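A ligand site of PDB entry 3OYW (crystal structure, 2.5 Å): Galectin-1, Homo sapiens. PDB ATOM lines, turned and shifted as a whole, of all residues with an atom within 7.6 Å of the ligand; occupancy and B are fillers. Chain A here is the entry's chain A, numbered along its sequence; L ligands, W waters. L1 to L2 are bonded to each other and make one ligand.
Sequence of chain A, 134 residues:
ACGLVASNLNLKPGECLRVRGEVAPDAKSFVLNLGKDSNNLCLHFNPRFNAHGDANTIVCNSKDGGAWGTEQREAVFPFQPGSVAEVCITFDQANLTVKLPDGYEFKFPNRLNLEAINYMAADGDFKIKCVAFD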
ATOM      1  N   VAL A  31       4.770  20.113 -18.573  1.00  0.00           N
ATOM      2  CA  VAL A  31       4.460  18.739 -18.942  1.00  0.00           C
ATOM      3  C   VAL A  31       5.448  17.766 -18.333  1.00  0.00           C
ATOM      4  O   VAL A  31       6.657  17.947 -18.458  1.00  0.00           O
ATOM      5  CB  VAL A  31       4.461  18.575 -20.495  1.00  0.00           C
ATOM      6  CG1 VAL A  31       4.442  17.113 -20.897  1.00  0.00           C
ATOM      7  CG2 VAL A  31       3.267  19.310 -21.112  1.00  0.00           C
ATOM      8  N   ASN A  33       5.959  13.737 -18.937  1.00  0.00           N
ATOM      9  CA  ASN A  33       5.559  12.538 -19.644  1.00  0.00           C
ATOM     10  C   ASN A  33       6.325  11.336 -19.129  1.00  0.00           C
ATOM     11  O   ASN A  33       7.547  11.370 -19.024  1.00  0.00           O
ATOM     12  CB  ASN A  33       5.847  12.678 -21.144  1.00  0.00           C
ATOM     13  CG  ASN A  33       4.900  13.626 -21.840  1.00  0.00           C
ATOM     14  OD1 ASN A  33       3.747  13.781 -21.452  1.00  0.00           O
ATOM     15  ND2 ASN A  33       5.396  14.267 -22.881  1.00  0.00           N
ATOM     16  N   HIS A  44       0.726  11.381 -19.095  1.00  0.00           N
ATOM     17  CA  HIS A  44       1.003  12.712 -19.595  1.00  0.00           C
ATOM     18  C   HIS A  44       0.364  13.645 -18.559  1.00  0.00           C
ATOM     19  O   HIS A  44      -0.859  13.747 -18.467  1.00  0.00           O
ATOM     20  CB  HIS A  44       0.403  12.867 -20.998  1.00  0.00           C
ATOM     21  CG  HIS A  44       0.345  14.273 -21.490  1.00  0.00           C
ATOM     22  ND1 HIS A  44       1.409  14.901 -22.102  1.00  0.00           N
ATOM     23  CD2 HIS A  44      -0.660  15.183 -21.466  1.00  0.00           C
ATOM     24  CE1 HIS A  44       1.064  16.134 -22.429  1.00  0.00           C
ATOM     25  NE2 HIS A  44      -0.175  16.338 -22.051  1.00  0.00           N
ATOM     26  N   PHE A  45       1.209  14.289 -17.759  1.00  0.00           N
ATOM     27  CA  PHE A  45       0.778  15.123 -16.635  1.00  0.00           C
ATOM     28  C   PHE A  45       0.982  16.561 -17.044  1.00  0.00           C
ATOM     29  O   PHE A  45       2.122  17.014 -17.238  1.00  0.00           O
ATOM     30  CB  PHE A  45       1.649  14.807 -15.422  1.00  0.00           C
ATOM     31  CG  PHE A  45       1.357  15.635 -14.195  1.00  0.00           C
ATOM     32  CD1 PHE A  45       0.244  15.369 -13.404  1.00  0.00           C
ATOM     33  CD2 PHE A  45       2.236  16.637 -13.800  1.00  0.00           C
ATOM     34  CE1 PHE A  45      -0.014  16.096 -12.251  1.00  0.00           C
ATOM     35  CE2 PHE A  45       2.002  17.384 -12.629  1.00  0.00           C
ATOM     36  CZ  PHE A  45       0.866  17.111 -11.857  1.00  0.00           C
ATOM     37  N   ASN A  46      -0.126  17.281 -17.197  1.00  0.00           N
ATOM     38  CA  ASN A  46      -0.074  18.588 -17.826  1.00  0.00           C
ATOM     39  C   ASN A  46      -0.840  19.676 -17.053  1.00  0.00           C
ATOM     40  O   ASN A  46      -2.004  19.976 -17.371  1.00  0.00           O
ATOM     41  CB  ASN A  46      -0.547  18.449 -19.284  1.00  0.00           C
ATOM     42  CG  ASN A  46      -0.575  19.760 -20.042  1.00  0.00           C
ATOM     43  OD1 ASN A  46      -1.448  19.964 -20.876  1.00  0.00           O
ATOM     44  ND2 ASN A  46       0.393  20.637 -19.767  1.00  0.00           N
ATOM     45  N   ARG A  48      -2.140  23.075 -16.444  1.00  0.00           N
ATOM     46  CA  ARG A  48      -2.366  24.218 -17.322  1.00  0.00           C
ATOM     47  C   ARG A  48      -2.761  25.451 -16.513  1.00  0.00           C
ATOM     48  O   ARG A  48      -3.851  25.506 -15.960  1.00  0.00           O
ATOM     49  CB  ARG A  48      -3.450  23.898 -18.373  1.00  0.00           C
ATOM     50  CG  ARG A  48      -3.001  22.876 -19.408  1.00  0.00           C
ATOM     51  CD  ARG A  48      -4.155  22.447 -20.302  1.00  0.00           C
ATOM     52  NE  ARG A  48      -3.793  21.294 -21.121  1.00  0.00           N
ATOM     53  CZ  ARG A  48      -4.578  20.734 -22.046  1.00  0.00           C
ATOM     54  NH1 ARG A  48      -5.789  21.228 -22.303  1.00  0.00           N
ATOM     55  NH2 ARG A  48      -4.134  19.684 -22.723  1.00  0.00           N
ATOM     56  N   ALA A  51      -3.714  27.674 -20.797  1.00  0.00           N
ATOM     57  CA  ALA A  51      -3.428  27.027 -22.079  1.00  0.00           C
ATOM     58  C   ALA A  51      -4.608  26.204 -22.559  1.00  0.00           C
ATOM     59  O   ALA A  51      -5.321  25.595 -21.744  1.00  0.00           O
ATOM     60  CB  ALA A  51      -2.166  26.166 -21.979  1.00  0.00           C
ATOM     61  N   HIS A  52      -4.815  26.192 -23.878  1.00  0.00           N
ATOM     62  CA  HIS A  52      -5.902  25.453 -24.551  1.00  0.00           C
ATOM     63  C   HIS A  52      -7.306  25.806 -24.019  1.00  0.00           C
ATOM     64  O   HIS A  52      -8.196  24.953 -23.982  1.00  0.00           O
ATOM     65  CB  HIS A  52      -5.668  23.932 -24.486  1.00  0.00           C
ATOM     66  CG  HIS A  52      -4.403  23.490 -25.134  1.00  0.00           C
ATOM     67  ND1 HIS A  52      -3.228  23.304 -24.441  1.00  0.00           N
ATOM     68  CD2 HIS A  52      -4.114  23.184 -26.426  1.00  0.00           C
ATOM     69  CE1 HIS A  52      -2.275  22.913 -25.272  1.00  0.00           C
ATOM     70  NE2 HIS A  52      -2.793  22.833 -26.481  1.00  0.00           N
ATOM     71  N   ASP A  54      -8.196  26.302 -21.024  1.00  0.00           N
ATOM     72  CA  ASP A  54      -8.208  25.966 -19.598  1.00  0.00           C
ATOM     73  C   ASP A  54      -7.434  26.930 -18.708  1.00  0.00           C
ATOM     74  O   ASP A  54      -6.428  27.529 -19.121  1.00  0.00           O
ATOM     75  CB  ASP A  54      -7.649  24.554 -19.385  1.00  0.00           C
ATOM     76  CG  ASP A  54      -8.363  23.531 -20.219  1.00  0.00           C
ATOM     77  OD1 ASP A  54      -9.565  23.725 -20.484  1.00  0.00           O
ATOM     78  OD2 ASP A  54      -7.730  22.516 -20.588  1.00  0.00           O
ATOM     79  N   VAL A  59      -4.459  18.483 -16.407  1.00  0.00           N
ATOM     80  CA  VAL A  59      -4.962  17.623 -17.456  1.00  0.00           C
ATOM     81  C   VAL A  59      -4.068  16.396 -17.569  1.00  0.00           C
ATOM     82  O   VAL A  59      -2.859  16.523 -17.754  1.00  0.00           O
ATOM     83  CB  VAL A  59      -5.054  18.374 -18.802  1.00  0.00           C
ATOM     84  CG1 VAL A  59      -5.206  17.407 -19.981  1.00  0.00           C
ATOM     85  CG2 VAL A  59      -6.219  19.373 -18.757  1.00  0.00           C
ATOM     86  N   CYS A  60      -4.670  15.217 -17.428  1.00  0.00           N
ATOM     87  CA  CYS A  60      -3.948  13.946 -17.502  1.00  0.00           C
ATOM     88  C   CYS A  60      -4.449  13.092 -18.651  1.00  0.00           C
ATOM     89  O   CYS A  60      -5.647  13.035 -18.934  1.00  0.00           O
ATOM     90  CB  CYS A  60      -4.085  13.163 -16.197  1.00  0.00           C
ATOM     91  SG  CYS A  60      -3.163  13.777 -14.776  1.00  0.00           S
ATOM     92  N   ASN A  61      -3.522  12.417 -19.318  1.00  0.00           N
ATOM     93  CA  ASN A  61      -3.872  11.498 -20.390  1.00  0.00           C
ATOM     94  C   ASN A  61      -2.816  10.422 -20.570  1.00  0.00           C
ATOM     95  O   ASN A  61      -1.796  10.406 -19.889  1.00  0.00           O
ATOM     96  CB  ASN A  61      -4.101  12.265 -21.711  1.00  0.00           C
ATOM     97  CG  ASN A  61      -5.119  11.587 -22.607  1.00  0.00           C
ATOM     98  OD1 ASN A  61      -5.528  10.441 -22.357  1.00  0.00           O
ATOM     99  ND2 ASN A  61      -5.555  12.281 -23.650  1.00  0.00           N
ATOM    100  N   SER A  62      -3.083   9.519 -21.509  1.00  0.00           N
ATOM    101  CA  SER A  62      -2.108   8.531 -21.930  1.00  0.00           C
ATOM    102  C   SER A  62      -1.982   8.579 -23.446  1.00  0.00           C
ATOM    103  O   SER A  62      -2.765   9.242 -24.121  1.00  0.00           O
ATOM    104  CB  SER A  62      -2.527   7.125 -21.469  1.00  0.00           C
ATOM    105  OG  SER A  62      -3.858   6.856 -21.882  1.00  0.00           O
ATOM    106  N   LYS A  63      -0.985   7.875 -23.953  1.00  0.00           N
ATOM    107  CA  LYS A  63      -0.704   7.787 -25.373  1.00  0.00           C
ATOM    108  C   LYS A  63      -0.286   6.345 -25.636  1.00  0.00           C
ATOM    109  O   LYS A  63       0.601   5.814 -24.964  1.00  0.00           O
ATOM    110  CB  LYS A  63       0.415   8.763 -25.737  1.00  0.00           C
ATOM    111  CG  LYS A  63       0.555   9.033 -27.233  1.00  0.00           C
ATOM    112  CD  LYS A  63       1.667  10.040 -27.478  1.00  0.00           C
ATOM    113  CE  LYS A  63       1.207  11.122 -28.424  1.00  0.00           C
ATOM    114  NZ  LYS A  63       2.083  12.322 -28.320  1.00  0.00           N
ATOM    115  N   TRP A  68      -3.547   9.481 -28.424  1.00  0.00           N
ATOM    116  CA  TRP A  68      -4.050   9.991 -27.157  1.00  0.00           C
ATOM    117  C   TRP A  68      -5.233   9.167 -26.648  1.00  0.00           C
ATOM    118  O   TRP A  68      -6.118   8.799 -27.421  1.00  0.00           O
ATOM    119  CB  TRP A  68      -4.468  11.451 -27.300  1.00  0.00           C
ATOM    120  CG  TRP A  68      -3.320  12.416 -27.410  1.00  0.00           C
ATOM    121  CD1 TRP A  68      -3.054  13.265 -28.446  1.00  0.00           C
ATOM    122  CD2 TRP A  68      -2.291  12.651 -26.434  1.00  0.00           C
ATOM    123  NE1 TRP A  68      -1.929  14.005 -28.182  1.00  0.00           N
ATOM    124  CE2 TRP A  68      -1.434  13.647 -26.955  1.00  0.00           C
ATOM    125  CE3 TRP A  68      -2.013  12.110 -25.169  1.00  0.00           C
ATOM    126  CZ2 TRP A  68      -0.303  14.114 -26.253  1.00  0.00           C
ATOM    127  CZ3 TRP A  68      -0.891  12.578 -24.466  1.00  0.00           C
ATOM    128  CH2 TRP A  68      -0.058  13.567 -25.020  1.00  0.00           C
ATOM    129  N   GLY A  69      -5.247   8.893 -25.340  1.00  0.00           N
ATOM    130  CA  GLY A  69      -6.377   8.201 -24.717  1.00  0.00           C
ATOM    131  C   GLY A  69      -7.476   9.191 -24.335  1.00  0.00           C
ATOM    132  O   GLY A  69      -7.452  10.346 -24.752  1.00  0.00           O
ATOM    133  N   THR A  70      -8.428   8.717 -23.536  1.00  0.00           N
ATOM    134  CA  THR A  70      -9.444   9.559 -22.924  1.00  0.00           C
ATOM    135  C   THR A  70      -8.823  10.460 -21.852  1.00  0.00           C
ATOM    136  O   THR A  70      -8.122  10.000 -20.949  1.00  0.00           O
ATOM    137  CB  THR A  70     -10.557   8.705 -22.270  1.00  0.00           C
ATOM    138  OG1 THR A  70     -10.994   7.713 -23.194  1.00  0.00           O
ATOM    139  CG2 THR A  70     -11.746   9.584 -21.865  1.00  0.00           C
ATOM    140  N   GLU A  71      -9.104  11.753 -21.967  1.00  0.00           N
ATOM    141  CA  GLU A  71      -8.548  12.785 -21.113  1.00  0.00           C
ATOM    142  C   GLU A  71      -9.268  12.867 -19.754  1.00  0.00           C
ATOM    143  O   GLU A  71     -10.482  12.682 -19.686  1.00  0.00           O
ATOM    144  CB  GLU A  71      -8.700  14.121 -21.812  1.00  0.00           C
ATOM    145  CG  GLU A  71      -7.560  15.041 -21.590  1.00  0.00           C
ATOM    146  CD  GLU A  71      -7.830  16.398 -22.152  1.00  0.00           C
ATOM    147  OE1 GLU A  71      -8.589  17.174 -21.529  1.00  0.00           O
ATOM    148  OE2 GLU A  71      -7.258  16.709 -23.212  1.00  0.00           O
ATOM    149  N   GLN A  72      -8.502  13.126 -18.693  1.00  0.00           N
ATOM    150  CA  GLN A  72      -9.048  13.347 -17.345  1.00  0.00           C
ATOM    151  C   GLN A  72      -8.555  14.638 -16.730  1.00  0.00           C
ATOM    152  O   GLN A  72      -7.379  14.994 -16.850  1.00  0.00           O
ATOM    153  CB  GLN A  72      -8.687  12.196 -16.407  1.00  0.00           C
ATOM    154  CG  GLN A  72      -9.578  10.994 -16.566  1.00  0.00           C
ATOM    155  CD  GLN A  72      -9.205   9.862 -15.637  1.00  0.00           C
ATOM    156  OE1 GLN A  72      -9.572   8.717 -15.874  1.00  0.00           O
ATOM    157  NE2 GLN A  72      -8.482  10.176 -14.555  1.00  0.00           N
ATOM    158  N   ARG A  73      -9.459  15.339 -16.053  1.00  0.00           N
ATOM    159  CA  ARG A  73      -9.086  16.557 -15.331  1.00  0.00           C
ATOM    160  C   ARG A  73      -9.194  16.393 -13.823  1.00  0.00           C
ATOM    161  O   ARG A  73     -10.143  15.789 -13.322  1.00  0.00           O
ATOM    162  CB  ARG A  73      -9.901  17.750 -15.827  1.00  0.00           C
ATOM    163  CG  ARG A  73      -9.413  18.242 -17.156  1.00  0.00           C
ATOM    164  CD  ARG A  73     -10.524  18.801 -18.016  1.00  0.00           C
ATOM    165  NE  ARG A  73     -10.016  19.003 -19.369  1.00  0.00           N
ATOM    166  CZ  ARG A  73      -9.653  20.184 -19.867  1.00  0.00           C
ATOM    167  NH1 ARG A  73      -9.785  21.293 -19.136  1.00  0.00           N
ATOM    168  NH2 ARG A  73      -9.189  20.271 -21.109  1.00  0.00           N
HETATM  169  C1  LIG L   1      -4.100  18.419 -26.124  1.00  0.00           C
HETATM  170  C2  LIG L   1      -2.656  18.962 -26.159  1.00  0.00           C
HETATM  171  C3  LIG L   1      -1.666  17.816 -25.937  1.00  0.00           C
HETATM  172  C4  LIG L   1      -2.005  17.050 -24.659  1.00  0.00           C
HETATM  173  C5  LIG L   1      -3.432  16.513 -24.804  1.00  0.00           C
HETATM  174  C6  LIG L   1      -3.840  15.646 -23.627  1.00  0.00           C
HETATM  175  O1  LIG L   1      -2.380  19.580 -27.407  1.00  0.00           O
HETATM  176  O2  LIG L   1      -0.321  18.306 -25.875  1.00  0.00           O
HETATM  177  O3  LIG L   1      -1.917  17.921 -23.525  1.00  0.00           O
HETATM  178  O4  LIG L   1      -4.316  17.641 -24.934  1.00  0.00           O
HETATM  179  O5  LIG L   1      -5.144  15.097 -23.860  1.00  0.00           O
HETATM  180  S1  LIG L   1      -5.272  19.743 -26.193  1.00  0.00           S
HETATM  181  C1  LG2 L   2      -6.747  18.764 -26.125  1.00  0.00           C
HETATM  182  C2  LG2 L   2      -7.789  19.352 -25.150  1.00  0.00           C
HETATM  183  C3  LG2 L   2      -9.068  18.509 -25.187  1.00  0.00           C
HETATM  184  C4  LG2 L   2      -9.562  18.245 -26.620  1.00  0.00           C
HETATM  185  C5  LG2 L   2      -8.404  17.692 -27.457  1.00  0.00           C
HETATM  186  C6  LG2 L   2      -8.839  17.309 -28.887  1.00  0.00           C
HETATM  187  O1  LG2 L   2      -7.288  19.359 -23.807  1.00  0.00           O
HETATM  188  O2  LG2 L   2     -10.104  19.123 -24.428  1.00  0.00           O
HETATM  189  O3  LG2 L   2     -10.038  19.464 -27.197  1.00  0.00           O
HETATM  190  O4  LG2 L   2      -7.318  18.637 -27.439  1.00  0.00           O
HETATM  191  O5  LG2 L   2      -8.357  18.249 -29.855  1.00  0.00           O
HETATM  192  O   HOH W   1      -6.567  14.892 -26.397  1.00  0.00           O
HETATM  193  O   HOH W   2       0.327  20.609 -23.594  1.00  0.00           O
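Water W2 lies within hydrogen-bond range of an oxygen (O2) of LIG L1 and the side-chain amide oxygen of Asn 46.
Merely in contact with the ligand: Trp 68 (3.7 Å). Hydrophobic or aromatic side chains that line the ligand: His 44, His 52 and Trp 68. Eight residues have an atom within 4 Å of the ligand: His 44, Asn 46, Arg 48, His 52, Asn 61, Trp 68, Glu 71 and Arg 73.
O1 of LG2 L2 sits at hydrogen-bond distance from OE2 of Glu 71 (2.7 Å). A ring nitrogen (NE2) of His 44 lies within hydrogen-bond range of an oxygen (O3) of LIG L1. The guanidinium group (NH1) of Arg 48 lies within hydrogen-bond range of an oxygen (O1) of LG2 L2 (2.8 Å). O5 of LIG L1 sits at hydrogen-bond distance from ND2 of Asn 61 (2.9 Å). The side-chain amide oxygen of Asn 46 sits at hydrogen-bond distance from an oxygen (O3) of LIG L1 (3.4 Å). A ring nitrogen (NE2) of His 52 lies within hydrogen-bond range of an oxygen (O1) of LIG L1, 3.4 Å away. An oxygen (O1) of LG2 L2 sits at hydrogen-bond distance from the guanidinium group of Arg 73 (3.4 Å).
The side-chain carboxylate of Glu 71 lies within salt-bridge range of the guanidinium group of Arg 73 (3.2 Å). The backbone NH of His 44 lies within hydrogen-bond range of the backbone carbonyl oxygen of Asn 61 (2.8 Å). OD1 of Asn 33 lies within hydrogen-bond range of ND1 of His 44, 2.7 Å away. NE of Arg 48 is in hydrogen-bond range of OD1 of Asn 46 (2.7 Å). NH1 of Arg 48 is in salt-bridge range of OD2 of Asp 54 (2.9 Å). O of Gly 69 sits at hydrogen-bond distance from ND2 of Asn 61 (2.9 Å). The side-chain amide oxygen (OD1) of Asn 61 sits close to the backbone carbonyl oxygen (O) of Thr 70 (3.0 Å). NH2 of Arg 73 lies within salt-bridge range of OD2 of Asp 54, at 2.7 Å.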
